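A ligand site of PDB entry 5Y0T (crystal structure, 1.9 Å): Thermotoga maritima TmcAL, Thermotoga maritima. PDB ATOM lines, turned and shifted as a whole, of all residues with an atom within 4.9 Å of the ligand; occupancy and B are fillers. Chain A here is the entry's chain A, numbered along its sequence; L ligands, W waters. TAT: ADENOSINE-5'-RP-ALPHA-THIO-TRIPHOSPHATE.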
ATOM      1  N   VAL A   7       3.259 -25.075 -19.631  1.00  0.00           N
ATOM      2  CA  VAL A   7       1.949 -25.625 -19.978  1.00  0.00           C
ATOM      3  C   VAL A   7       1.533 -25.008 -21.294  1.00  0.00           C
ATOM      4  O   VAL A   7       1.477 -23.789 -21.405  1.00  0.00           O
ATOM      5  CB  VAL A   7       0.896 -25.292 -18.903  1.00  0.00           C
ATOM      6  CG1 VAL A   7      -0.492 -25.874 -19.309  1.00  0.00           C
ATOM      7  CG2 VAL A   7       1.353 -25.829 -17.540  1.00  0.00           C
ATOM      8  N   VAL A   8       1.285 -25.834 -22.320  1.00  0.00           N
ATOM      9  CA  VAL A   8       1.157 -25.296 -23.671  1.00  0.00           C
ATOM     10  C   VAL A   8       0.137 -26.057 -24.494  1.00  0.00           C
ATOM     11  O   VAL A   8      -0.245 -27.170 -24.169  1.00  0.00           O
ATOM     12  CB  VAL A   8       2.522 -25.333 -24.443  1.00  0.00           C
ATOM     13  CG1 VAL A   8       3.598 -24.545 -23.692  1.00  0.00           C
ATOM     14  CG2 VAL A   8       2.973 -26.786 -24.645  1.00  0.00           C
ATOM     15  N   GLU A   9      -0.286 -25.434 -25.586  1.00  0.00           N
ATOM     16  CA  GLU A   9      -1.205 -26.036 -26.547  1.00  0.00           C
ATOM     17  C   GLU A   9      -0.546 -25.976 -27.932  1.00  0.00           C
ATOM     18  O   GLU A   9      -0.620 -26.938 -28.687  1.00  0.00           O
ATOM     19  CB  GLU A   9      -2.572 -25.363 -26.502  1.00  0.00           C
ATOM     20  CG  GLU A   9      -3.252 -25.653 -25.177  1.00  0.00           C
ATOM     21  CD  GLU A   9      -4.760 -25.590 -25.270  1.00  0.00           C
ATOM     22  OE1 GLU A   9      -5.273 -24.522 -25.630  1.00  0.00           O
ATOM     23  OE2 GLU A   9      -5.427 -26.618 -25.008  1.00  0.00           O
ATOM     24  N   TYR A  10      -0.013 -24.807 -28.284  1.00  0.00           N
ATOM     25  CA  TYR A  10       0.748 -24.643 -29.532  1.00  0.00           C
ATOM     26  C   TYR A  10      -0.130 -24.988 -30.730  1.00  0.00           C
ATOM     27  O   TYR A  10       0.196 -25.884 -31.501  1.00  0.00           O
ATOM     28  CB  TYR A  10       2.017 -25.532 -29.519  1.00  0.00           C
ATOM     29  CG  TYR A  10       3.119 -25.125 -28.549  1.00  0.00           C
ATOM     30  CD1 TYR A  10       3.202 -23.807 -28.063  1.00  0.00           C
ATOM     31  CD2 TYR A  10       4.081 -26.027 -28.127  1.00  0.00           C
ATOM     32  CE1 TYR A  10       4.228 -23.427 -27.181  1.00  0.00           C
ATOM     33  CE2 TYR A  10       5.103 -25.663 -27.251  1.00  0.00           C
ATOM     34  CZ  TYR A  10       5.176 -24.363 -26.778  1.00  0.00           C
ATOM     35  OH  TYR A  10       6.203 -24.000 -25.920  1.00  0.00           O
ATOM     36  N   HIS A  14       3.479 -20.412 -32.579  1.00  0.00           N
ATOM     37  CA  HIS A  14       3.669 -19.168 -33.322  1.00  0.00           C
ATOM     38  C   HIS A  14       4.748 -18.301 -32.680  1.00  0.00           C
ATOM     39  O   HIS A  14       5.438 -18.732 -31.771  1.00  0.00           O
ATOM     40  CB  HIS A  14       2.347 -18.384 -33.461  1.00  0.00           C
ATOM     41  CG  HIS A  14       1.624 -18.118 -32.175  1.00  0.00           C
ATOM     42  ND1 HIS A  14       2.257 -17.626 -31.040  1.00  0.00           N
ATOM     43  CD2 HIS A  14       0.319 -18.249 -31.839  1.00  0.00           C
ATOM     44  CE1 HIS A  14       1.362 -17.471 -30.074  1.00  0.00           C
ATOM     45  NE2 HIS A  14       0.182 -17.847 -30.535  1.00  0.00           N
ATOM     46  N   GLY A  16       4.555 -15.692 -30.799  1.00  0.00           N
ATOM     47  CA  GLY A  16       4.275 -15.396 -29.405  1.00  0.00           C
ATOM     48  C   GLY A  16       4.737 -16.534 -28.514  1.00  0.00           C
ATOM     49  O   GLY A  16       5.276 -16.333 -27.424  1.00  0.00           O
ATOM     50  N   HIS A  17       4.537 -17.756 -28.996  1.00  0.00           N
ATOM     51  CA  HIS A  17       4.981 -18.919 -28.245  1.00  0.00           C
ATOM     52  C   HIS A  17       6.506 -18.987 -28.165  1.00  0.00           C
ATOM     53  O   HIS A  17       7.058 -19.381 -27.148  1.00  0.00           O
ATOM     54  CB  HIS A  17       4.453 -20.185 -28.890  1.00  0.00           C
ATOM     55  CG  HIS A  17       2.966 -20.327 -28.815  1.00  0.00           C
ATOM     56  ND1 HIS A  17       2.194 -20.765 -29.873  1.00  0.00           N
ATOM     57  CD2 HIS A  17       2.106 -20.085 -27.798  1.00  0.00           C
ATOM     58  CE1 HIS A  17       0.931 -20.802 -29.507  1.00  0.00           C
ATOM     59  NE2 HIS A  17       0.849 -20.384 -28.256  1.00  0.00           N
ATOM     60  N   TYR A  19       8.432 -16.425 -28.203  1.00  0.00           N
ATOM     61  CA  TYR A  19       8.727 -15.320 -27.290  1.00  0.00           C
ATOM     62  C   TYR A  19       8.637 -15.762 -25.833  1.00  0.00           C
ATOM     63  O   TYR A  19       9.553 -15.514 -25.061  1.00  0.00           O
ATOM     64  CB  TYR A  19       7.764 -14.179 -27.581  1.00  0.00           C
ATOM     65  CG  TYR A  19       8.057 -12.857 -26.897  1.00  0.00           C
ATOM     66  CD1 TYR A  19       9.081 -12.030 -27.340  1.00  0.00           C
ATOM     67  CD2 TYR A  19       7.252 -12.423 -25.851  1.00  0.00           C
ATOM     68  CE1 TYR A  19       9.314 -10.812 -26.749  1.00  0.00           C
ATOM     69  CE2 TYR A  19       7.475 -11.185 -25.258  1.00  0.00           C
ATOM     70  CZ  TYR A  19       8.512 -10.392 -25.702  1.00  0.00           C
ATOM     71  OH  TYR A  19       8.715  -9.165 -25.101  1.00  0.00           O
ATOM     72  N   HIS A  20       7.536 -16.433 -25.481  1.00  0.00           N
ATOM     73  CA  HIS A  20       7.343 -16.991 -24.143  1.00  0.00           C
ATOM     74  C   HIS A  20       8.434 -17.991 -23.776  1.00  0.00           C
ATOM     75  O   HIS A  20       9.023 -17.939 -22.698  1.00  0.00           O
ATOM     76  CB  HIS A  20       5.988 -17.691 -24.050  1.00  0.00           C
ATOM     77  CG  HIS A  20       5.858 -18.599 -22.850  1.00  0.00           C
ATOM     78  ND1 HIS A  20       5.981 -19.967 -22.942  1.00  0.00           N
ATOM     79  CD2 HIS A  20       5.648 -18.316 -21.540  1.00  0.00           C
ATOM     80  CE1 HIS A  20       5.837 -20.497 -21.737  1.00  0.00           C
ATOM     81  NE2 HIS A  20       5.647 -19.515 -20.867  1.00  0.00           N
ATOM     82  N   VAL A 100       6.833 -21.182 -15.780  1.00  0.00           N
ATOM     83  CA  VAL A 100       6.661 -19.833 -16.280  1.00  0.00           C
ATOM     84  C   VAL A 100       5.453 -19.766 -17.223  1.00  0.00           C
ATOM     85  O   VAL A 100       5.375 -20.523 -18.189  1.00  0.00           O
ATOM     86  CB  VAL A 100       7.898 -19.355 -17.074  1.00  0.00           C
ATOM     87  CG1 VAL A 100       7.679 -17.946 -17.593  1.00  0.00           C
ATOM     88  CG2 VAL A 100       9.162 -19.423 -16.207  1.00  0.00           C
ATOM     89  N   PHE A 101       4.517 -18.862 -16.945  1.00  0.00           N
ATOM     90  CA  PHE A 101       3.381 -18.701 -17.858  1.00  0.00           C
ATOM     91  C   PHE A 101       3.247 -17.258 -18.311  1.00  0.00           C
ATOM     92  O   PHE A 101       3.599 -16.348 -17.579  1.00  0.00           O
ATOM     93  CB  PHE A 101       2.072 -19.173 -17.194  1.00  0.00           C
ATOM     94  CG  PHE A 101       1.787 -18.527 -15.863  1.00  0.00           C
ATOM     95  CD1 PHE A 101       2.110 -19.179 -14.675  1.00  0.00           C
ATOM     96  CD2 PHE A 101       1.157 -17.297 -15.777  1.00  0.00           C
ATOM     97  CE1 PHE A 101       1.852 -18.602 -13.442  1.00  0.00           C
ATOM     98  CE2 PHE A 101       0.889 -16.708 -14.553  1.00  0.00           C
ATOM     99  CZ  PHE A 101       1.246 -17.361 -13.380  1.00  0.00           C
ATOM    100  N   GLY A 102       2.725 -17.059 -19.527  1.00  0.00           N
ATOM    101  CA  GLY A 102       2.473 -15.730 -20.033  1.00  0.00           C
ATOM    102  C   GLY A 102       1.314 -15.097 -19.285  1.00  0.00           C
ATOM    103  O   GLY A 102       0.362 -15.781 -18.909  1.00  0.00           O
ATOM    104  N   SER A 103       1.407 -13.788 -19.064  1.00  0.00           N
ATOM    105  CA  SER A 103       0.481 -13.066 -18.206  1.00  0.00           C
ATOM    106  C   SER A 103       0.150 -11.688 -18.768  1.00  0.00           C
ATOM    107  O   SER A 103       1.028 -11.010 -19.310  1.00  0.00           O
ATOM    108  CB  SER A 103       1.088 -12.955 -16.794  1.00  0.00           C
ATOM    109  OG  SER A 103       0.495 -11.934 -16.019  1.00  0.00           O
ATOM    110  N   ASN A 168      -5.423 -15.332 -19.381  1.00  0.00           N
ATOM    111  CA  ASN A 168      -4.156 -15.961 -19.023  1.00  0.00           C
ATOM    112  C   ASN A 168      -3.815 -15.798 -17.544  1.00  0.00           C
ATOM    113  O   ASN A 168      -3.233 -16.709 -16.938  1.00  0.00           O
ATOM    114  CB  ASN A 168      -3.042 -15.429 -19.931  1.00  0.00           C
ATOM    115  CG  ASN A 168      -3.173 -15.931 -21.365  1.00  0.00           C
ATOM    116  OD1 ASN A 168      -2.729 -17.032 -21.684  1.00  0.00           O
ATOM    117  ND2 ASN A 168      -3.792 -15.136 -22.230  1.00  0.00           N
ATOM    118  N   ILE A 191       5.658 -14.051 -17.296  1.00  0.00           N
ATOM    119  CA  ILE A 191       6.269 -13.110 -18.231  1.00  0.00           C
ATOM    120  C   ILE A 191       5.150 -12.345 -18.910  1.00  0.00           C
ATOM    121  O   ILE A 191       4.024 -12.833 -19.016  1.00  0.00           O
ATOM    122  CB  ILE A 191       7.187 -13.822 -19.263  1.00  0.00           C
ATOM    123  CG1 ILE A 191       6.435 -14.903 -20.070  1.00  0.00           C
ATOM    124  CG2 ILE A 191       8.405 -14.416 -18.575  1.00  0.00           C
ATOM    125  CD1 ILE A 191       5.934 -14.426 -21.417  1.00  0.00           C
ATOM    126  N   LYS A 192       5.456 -11.123 -19.353  1.00  0.00           N
ATOM    127  CA  LYS A 192       4.452 -10.280 -19.978  1.00  0.00           C
ATOM    128  C   LYS A 192       4.048 -10.771 -21.369  1.00  0.00           C
ATOM    129  O   LYS A 192       4.910 -10.932 -22.235  1.00  0.00           O
ATOM    130  CB  LYS A 192       4.959  -8.838 -20.092  1.00  0.00           C
ATOM    131  CG  LYS A 192       3.939  -7.885 -20.738  1.00  0.00           C
ATOM    132  CD  LYS A 192       2.826  -7.495 -19.750  1.00  0.00           C
ATOM    133  CE  LYS A 192       1.825  -6.522 -20.392  1.00  0.00           C
ATOM    134  NZ  LYS A 192       0.903  -7.256 -21.335  1.00  0.00           N
ATOM    135  N   ARG A 193       2.760 -10.969 -21.613  1.00  0.00           N
ATOM    136  CA  ARG A 193       2.281 -11.219 -22.972  1.00  0.00           C
ATOM    137  C   ARG A 193       2.331  -9.959 -23.803  1.00  0.00           C
ATOM    138  O   ARG A 193       1.961  -8.891 -23.334  1.00  0.00           O
ATOM    139  CB  ARG A 193       0.852 -11.757 -22.974  1.00  0.00           C
ATOM    140  CG  ARG A 193       0.733 -13.165 -22.433  1.00  0.00           C
ATOM    141  CD  ARG A 193      -0.715 -13.601 -22.396  1.00  0.00           C
ATOM    142  NE  ARG A 193      -1.309 -13.569 -23.728  1.00  0.00           N
ATOM    143  CZ  ARG A 193      -1.466 -14.648 -24.497  1.00  0.00           C
ATOM    144  NH1 ARG A 193      -1.068 -15.838 -24.052  1.00  0.00           N
ATOM    145  NH2 ARG A 193      -2.021 -14.528 -25.700  1.00  0.00           N
ATOM    146  N   VAL A 194       2.782 -10.090 -25.057  1.00  0.00           N
ATOM    147  CA  VAL A 194       2.838  -8.960 -25.975  1.00  0.00           C
ATOM    148  C   VAL A 194       2.063  -9.231 -27.259  1.00  0.00           C
ATOM    149  O   VAL A 194       1.822 -10.385 -27.618  1.00  0.00           O
ATOM    150  CB  VAL A 194       4.294  -8.591 -26.339  1.00  0.00           C
ATOM    151  CG1 VAL A 194       5.123  -8.390 -25.080  1.00  0.00           C
ATOM    152  CG2 VAL A 194       4.908  -9.662 -27.225  1.00  0.00           C
ATOM    153  N   ALA A 196      -1.187  -9.581 -29.480  1.00  0.00           N
ATOM    154  CA  ALA A 196      -2.572  -9.950 -29.218  1.00  0.00           C
ATOM    155  C   ALA A 196      -2.668 -10.909 -28.031  1.00  0.00           C
ATOM    156  O   ALA A 196      -2.623 -12.127 -28.183  1.00  0.00           O
ATOM    157  CB  ALA A 196      -3.198 -10.582 -30.453  1.00  0.00           C
ATOM    158  N   PHE A 207       2.912 -10.566 -33.847  1.00  0.00           N
ATOM    159  CA  PHE A 207       2.291 -11.503 -32.932  1.00  0.00           C
ATOM    160  C   PHE A 207       0.785 -11.539 -33.145  1.00  0.00           C
ATOM    161  O   PHE A 207       0.045 -10.691 -32.653  1.00  0.00           O
ATOM    162  CB  PHE A 207       2.587 -11.106 -31.485  1.00  0.00           C
ATOM    163  CG  PHE A 207       4.039 -11.007 -31.163  1.00  0.00           C
ATOM    164  CD1 PHE A 207       4.733  -9.819 -31.347  1.00  0.00           C
ATOM    165  CD2 PHE A 207       4.721 -12.100 -30.655  1.00  0.00           C
ATOM    166  CE1 PHE A 207       6.076  -9.739 -31.032  1.00  0.00           C
ATOM    167  CE2 PHE A 207       6.067 -12.004 -30.334  1.00  0.00           C
ATOM    168  CZ  PHE A 207       6.741 -10.836 -30.522  1.00  0.00           C
ATOM    169  N   SER A 208       0.334 -12.577 -33.806  1.00  0.00           N
ATOM    170  CA  SER A 208      -1.083 -12.765 -34.010  1.00  0.00           C
ATOM    171  C   SER A 208      -1.429 -13.915 -33.105  1.00  0.00           C
ATOM    172  O   SER A 208      -0.572 -14.763 -32.840  1.00  0.00           O
ATOM    173  CB  SER A 208      -1.415 -13.063 -35.469  1.00  0.00           C
ATOM    174  OG  SER A 208      -1.236 -11.907 -36.271  1.00  0.00           O
ATOM    175  N   SER A 209      -2.651 -13.912 -32.583  1.00  0.00           N
ATOM    176  CA  SER A 209      -3.122 -14.987 -31.728  1.00  0.00           C
ATOM    177  C   SER A 209      -3.225 -16.289 -32.516  1.00  0.00           C
ATOM    178  O   SER A 209      -3.422 -16.282 -33.737  1.00  0.00           O
ATOM    179  CB  SER A 209      -4.494 -14.635 -31.143  1.00  0.00           C
ATOM    180  OG  SER A 209      -5.483 -14.704 -32.154  1.00  0.00           O
ATOM    181  N   ALA A 210      -3.136 -17.411 -31.808  1.00  0.00           N
ATOM    182  CA  ALA A 210      -3.312 -18.713 -32.423  1.00  0.00           C
ATOM    183  C   ALA A 210      -4.646 -18.797 -33.181  1.00  0.00           C
ATOM    184  O   ALA A 210      -4.720 -19.396 -34.254  1.00  0.00           O
ATOM    185  CB  ALA A 210      -3.213 -19.826 -31.345  1.00  0.00           C
ATOM    186  N   THR A 211      -5.687 -18.171 -32.643  1.00  0.00           N
ATOM    187  CA  THR A 211      -7.001 -18.234 -33.303  1.00  0.00           C
ATOM    188  C   THR A 211      -7.008 -17.396 -34.580  1.00  0.00           C
ATOM    189  O   THR A 211      -7.542 -17.817 -35.606  1.00  0.00           O
ATOM    190  CB  THR A 211      -8.140 -17.781 -32.353  1.00  0.00           C
ATOM    191  OG1 THR A 211      -8.217 -18.676 -31.230  1.00  0.00           O
ATOM    192  CG2 THR A 211      -9.482 -17.783 -33.076  1.00  0.00           C
HETATM  193  N1  TAT L   1       3.543 -13.177 -25.622  1.00  0.00           N
HETATM  194  C2  TAT L   1       4.037 -13.828 -24.542  1.00  0.00           C
HETATM  195  N3  TAT L   1       3.661 -15.062 -24.198  1.00  0.00           N
HETATM  196  C4  TAT L   1       2.755 -15.750 -24.939  1.00  0.00           C
HETATM  197  C5  TAT L   1       2.192 -15.128 -26.140  1.00  0.00           C
HETATM  198  C6  TAT L   1       2.653 -13.752 -26.452  1.00  0.00           C
HETATM  199  N6  TAT L   1       2.179 -13.090 -27.540  1.00  0.00           N
HETATM  200  N7  TAT L   1       1.346 -16.015 -26.680  1.00  0.00           N
HETATM  201  C8  TAT L   1       1.359 -17.134 -25.906  1.00  0.00           C
HETATM  202  N9  TAT L   1       2.202 -16.966 -24.868  1.00  0.00           N
HETATM  203  PA  TAT L   1      -0.567 -21.642 -25.360  1.00  0.00           P
HETATM  204  PB  TAT L   1      -2.317 -19.320 -25.752  1.00  0.00           P
HETATM  205  PG  TAT L   1      -3.153 -17.595 -27.918  1.00  0.00           P
HETATM  206  C1' TAT L   1       2.481 -17.955 -23.795  1.00  0.00           C
HETATM  207  O1A TAT L   1      -2.323 -17.062 -29.081  1.00  0.00           O
HETATM  208  O1B TAT L   1      -3.767 -19.653 -25.554  1.00  0.00           O
HETATM  209  S1G TAT L   1      -1.384 -22.262 -23.703  1.00  0.00           S
HETATM  210  C2' TAT L   1       1.182 -18.317 -23.080  1.00  0.00           C
HETATM  211  O2' TAT L   1       0.793 -17.310 -22.139  1.00  0.00           O
HETATM  212  O2A TAT L   1      -0.096 -22.700 -26.356  1.00  0.00           O
HETATM  213  O2B TAT L   1      -1.599 -18.524 -24.704  1.00  0.00           O
HETATM  214  O2G TAT L   1      -4.319 -18.441 -28.368  1.00  0.00           O
HETATM  215  C3' TAT L   1       1.533 -19.638 -22.444  1.00  0.00           C
HETATM  216  O3' TAT L   1       2.216 -19.451 -21.189  1.00  0.00           O
HETATM  217  O3A TAT L   1      -1.534 -20.665 -26.196  1.00  0.00           O
HETATM  218  O3B TAT L   1      -2.121 -18.604 -27.196  1.00  0.00           O
HETATM  219  O3G TAT L   1      -3.513 -16.590 -26.851  1.00  0.00           O
HETATM  220  C4' TAT L   1       2.508 -20.247 -23.461  1.00  0.00           C
HETATM  221  O4' TAT L   1       2.952 -19.186 -24.316  1.00  0.00           O
HETATM  222  C5' TAT L   1       1.844 -21.327 -24.318  1.00  0.00           C
HETATM  223  O5' TAT L   1       0.701 -20.746 -24.959  1.00  0.00           O
HETATM  224  O   HOH W   1      -5.200 -19.007 -23.548  1.00  0.00           O
HETATM  225  O   HOH W   2      -0.760 -15.172 -28.511  1.00  0.00           O
HETATM  226  O   HOH W   3      -6.248 -17.544 -29.715  1.00  0.00           O
HETATM  227  O   HOH W   4       1.272 -21.550 -19.903  1.00  0.00           O
HETATM  228  O   HOH W   5      -4.783 -16.687 -24.770  1.00  0.00           O
HETATM  229  O   HOH W   6      -1.868 -22.272 -28.923  1.00  0.00           O
HETATM  230  O   HOH W   7       1.218 -13.998 -30.004  1.00  0.00           O
HETATM  231  O   HOH W   8      -6.264 -18.954 -26.699  1.00  0.00           O
HETATM  232  O   HOH W   9      -5.070 -14.383 -27.390  1.00  0.00           O
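The side-chain amide oxygen (OD1) of Asn 168 lies within hydrogen-bond range of the guanidinium group (NH1) of Arg 193 (3.1 Å). The backbone NH of Arg 193 sits at hydrogen-bond distance from the backbone carbonyl oxygen of Ser 103, at 2.9 Å. The backbone NH of His 14 is in hydrogen-bond range of a ring nitrogen (ND1) of His 17, at 3.0 Å. The backbone NH (N) of Gly 16 sits at hydrogen-bond distance from a ring nitrogen (ND1) of His 14. A ring nitrogen (NE2) of His 20 sits at hydrogen-bond distance from the backbone carbonyl oxygen (O) of Val 100 (2.9 Å). O of Phe 101 lies within hydrogen-bond range of N of Ile 191 (3.1 Å). The backbone carbonyl oxygen (O) of Ile 191 lies within hydrogen-bond range of the backbone NH (N) of Ser 103 (2.8 Å).
Water W5 lies within hydrogen-bond range of O3G of the ligand (2.4 Å) and ND2 of Asn 168 (3.1 Å). Water W2 lies within hydrogen-bond range of an oxygen (O1A) of the ligand, the guanidinium group of Arg 193 and a ring nitrogen (NE2) of His 14. Water W3 lies within hydrogen-bond range of an oxygen (O2G) of the ligand and the side-chain hydroxyl (OG1) of Thr 211. Water W9 lies within hydrogen-bond range of O3G of the ligand, O of Ala 196 and NH2 of Arg 193. Water W7 bridges a nitrogen (N6) of the ligand and the backbone carbonyl oxygen of Ser 208. Water W6 lies within hydrogen-bond range of O2A of the ligand (3.1 Å), N of Tyr 10 (3.2 Å) and NE2 of His 17 (3.4 Å).
Val 7 touches the ligand. Val 8 touches the ligand (CG1 to C5', 3.7 Å). O of Gly 16 touches C5 of the ligand (3.6 Å). CD2 of Tyr 19 touches C2 of the ligand (3.7 Å). CA of Phe 101 touches O3' of the ligand, at 3.6 Å. OD1 of Asn 168 touches O2B of the ligand, 3.6 Å away. Ile 191 touches the ligand (CD1 to N3, 3.6 Å). Lys 192 touches the ligand. Ser 209 touches the ligand (CA to O1A, 3.5 Å). Hydrophobic or aromatic side chains within 4 Å of the ligand: Val 8, Tyr 10, His 14, His 17, Tyr 19, His 20, Ile 191 and Ala 210. 18 residues have an atom within 4 Å of the ligand: Val 7, Val 8, Glu 9, Tyr 10, His 14, Gly 16, His 17, Tyr 19, His 20, Phe 101, Gly 102, Asn 168, Ile 191, Lys 192, Arg 193, Val 194, Ser 209 and Ala 210. The nearest printed residue that does not touch the ligand is Phe 207 (4.1 Å).
A nitrogen (N1) of the ligand lies within hydrogen-bond range of the backbone NH of Val 194. The backbone carbonyl oxygen of Val 194 sits at hydrogen-bond distance from a nitrogen (N6) of the ligand (2.7 Å). An oxygen (O3G) of the ligand lies within salt-bridge range of the guanidinium group (NH2) of Arg 193 (2.8 Å). The backbone NH (N) of Glu 9 lies within hydrogen-bond range of an oxygen (O2A) of the ligand (2.8 Å). The backbone NH of Tyr 10 lies within hydrogen-bond range of an oxygen (O2A) of the ligand. O1A of the ligand lies within hydrogen-bond range of N of Ala 210, at 2.9 Å. An oxygen (O3') of the ligand lies within hydrogen-bond range of the backbone NH (N) of Gly 102 (3.0 Å). A ring nitrogen (NE2) of His 14 is in hydrogen-bond range of an oxygen (O1A) of the ligand, at 3.0 Å. A ring nitrogen (NE2) of His 17 sits at hydrogen-bond distance from an oxygen (O2A) of the ligand (3.1 Å). An oxygen (O4') of the ligand lies close to a ring nitrogen (ND1) of His 20.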
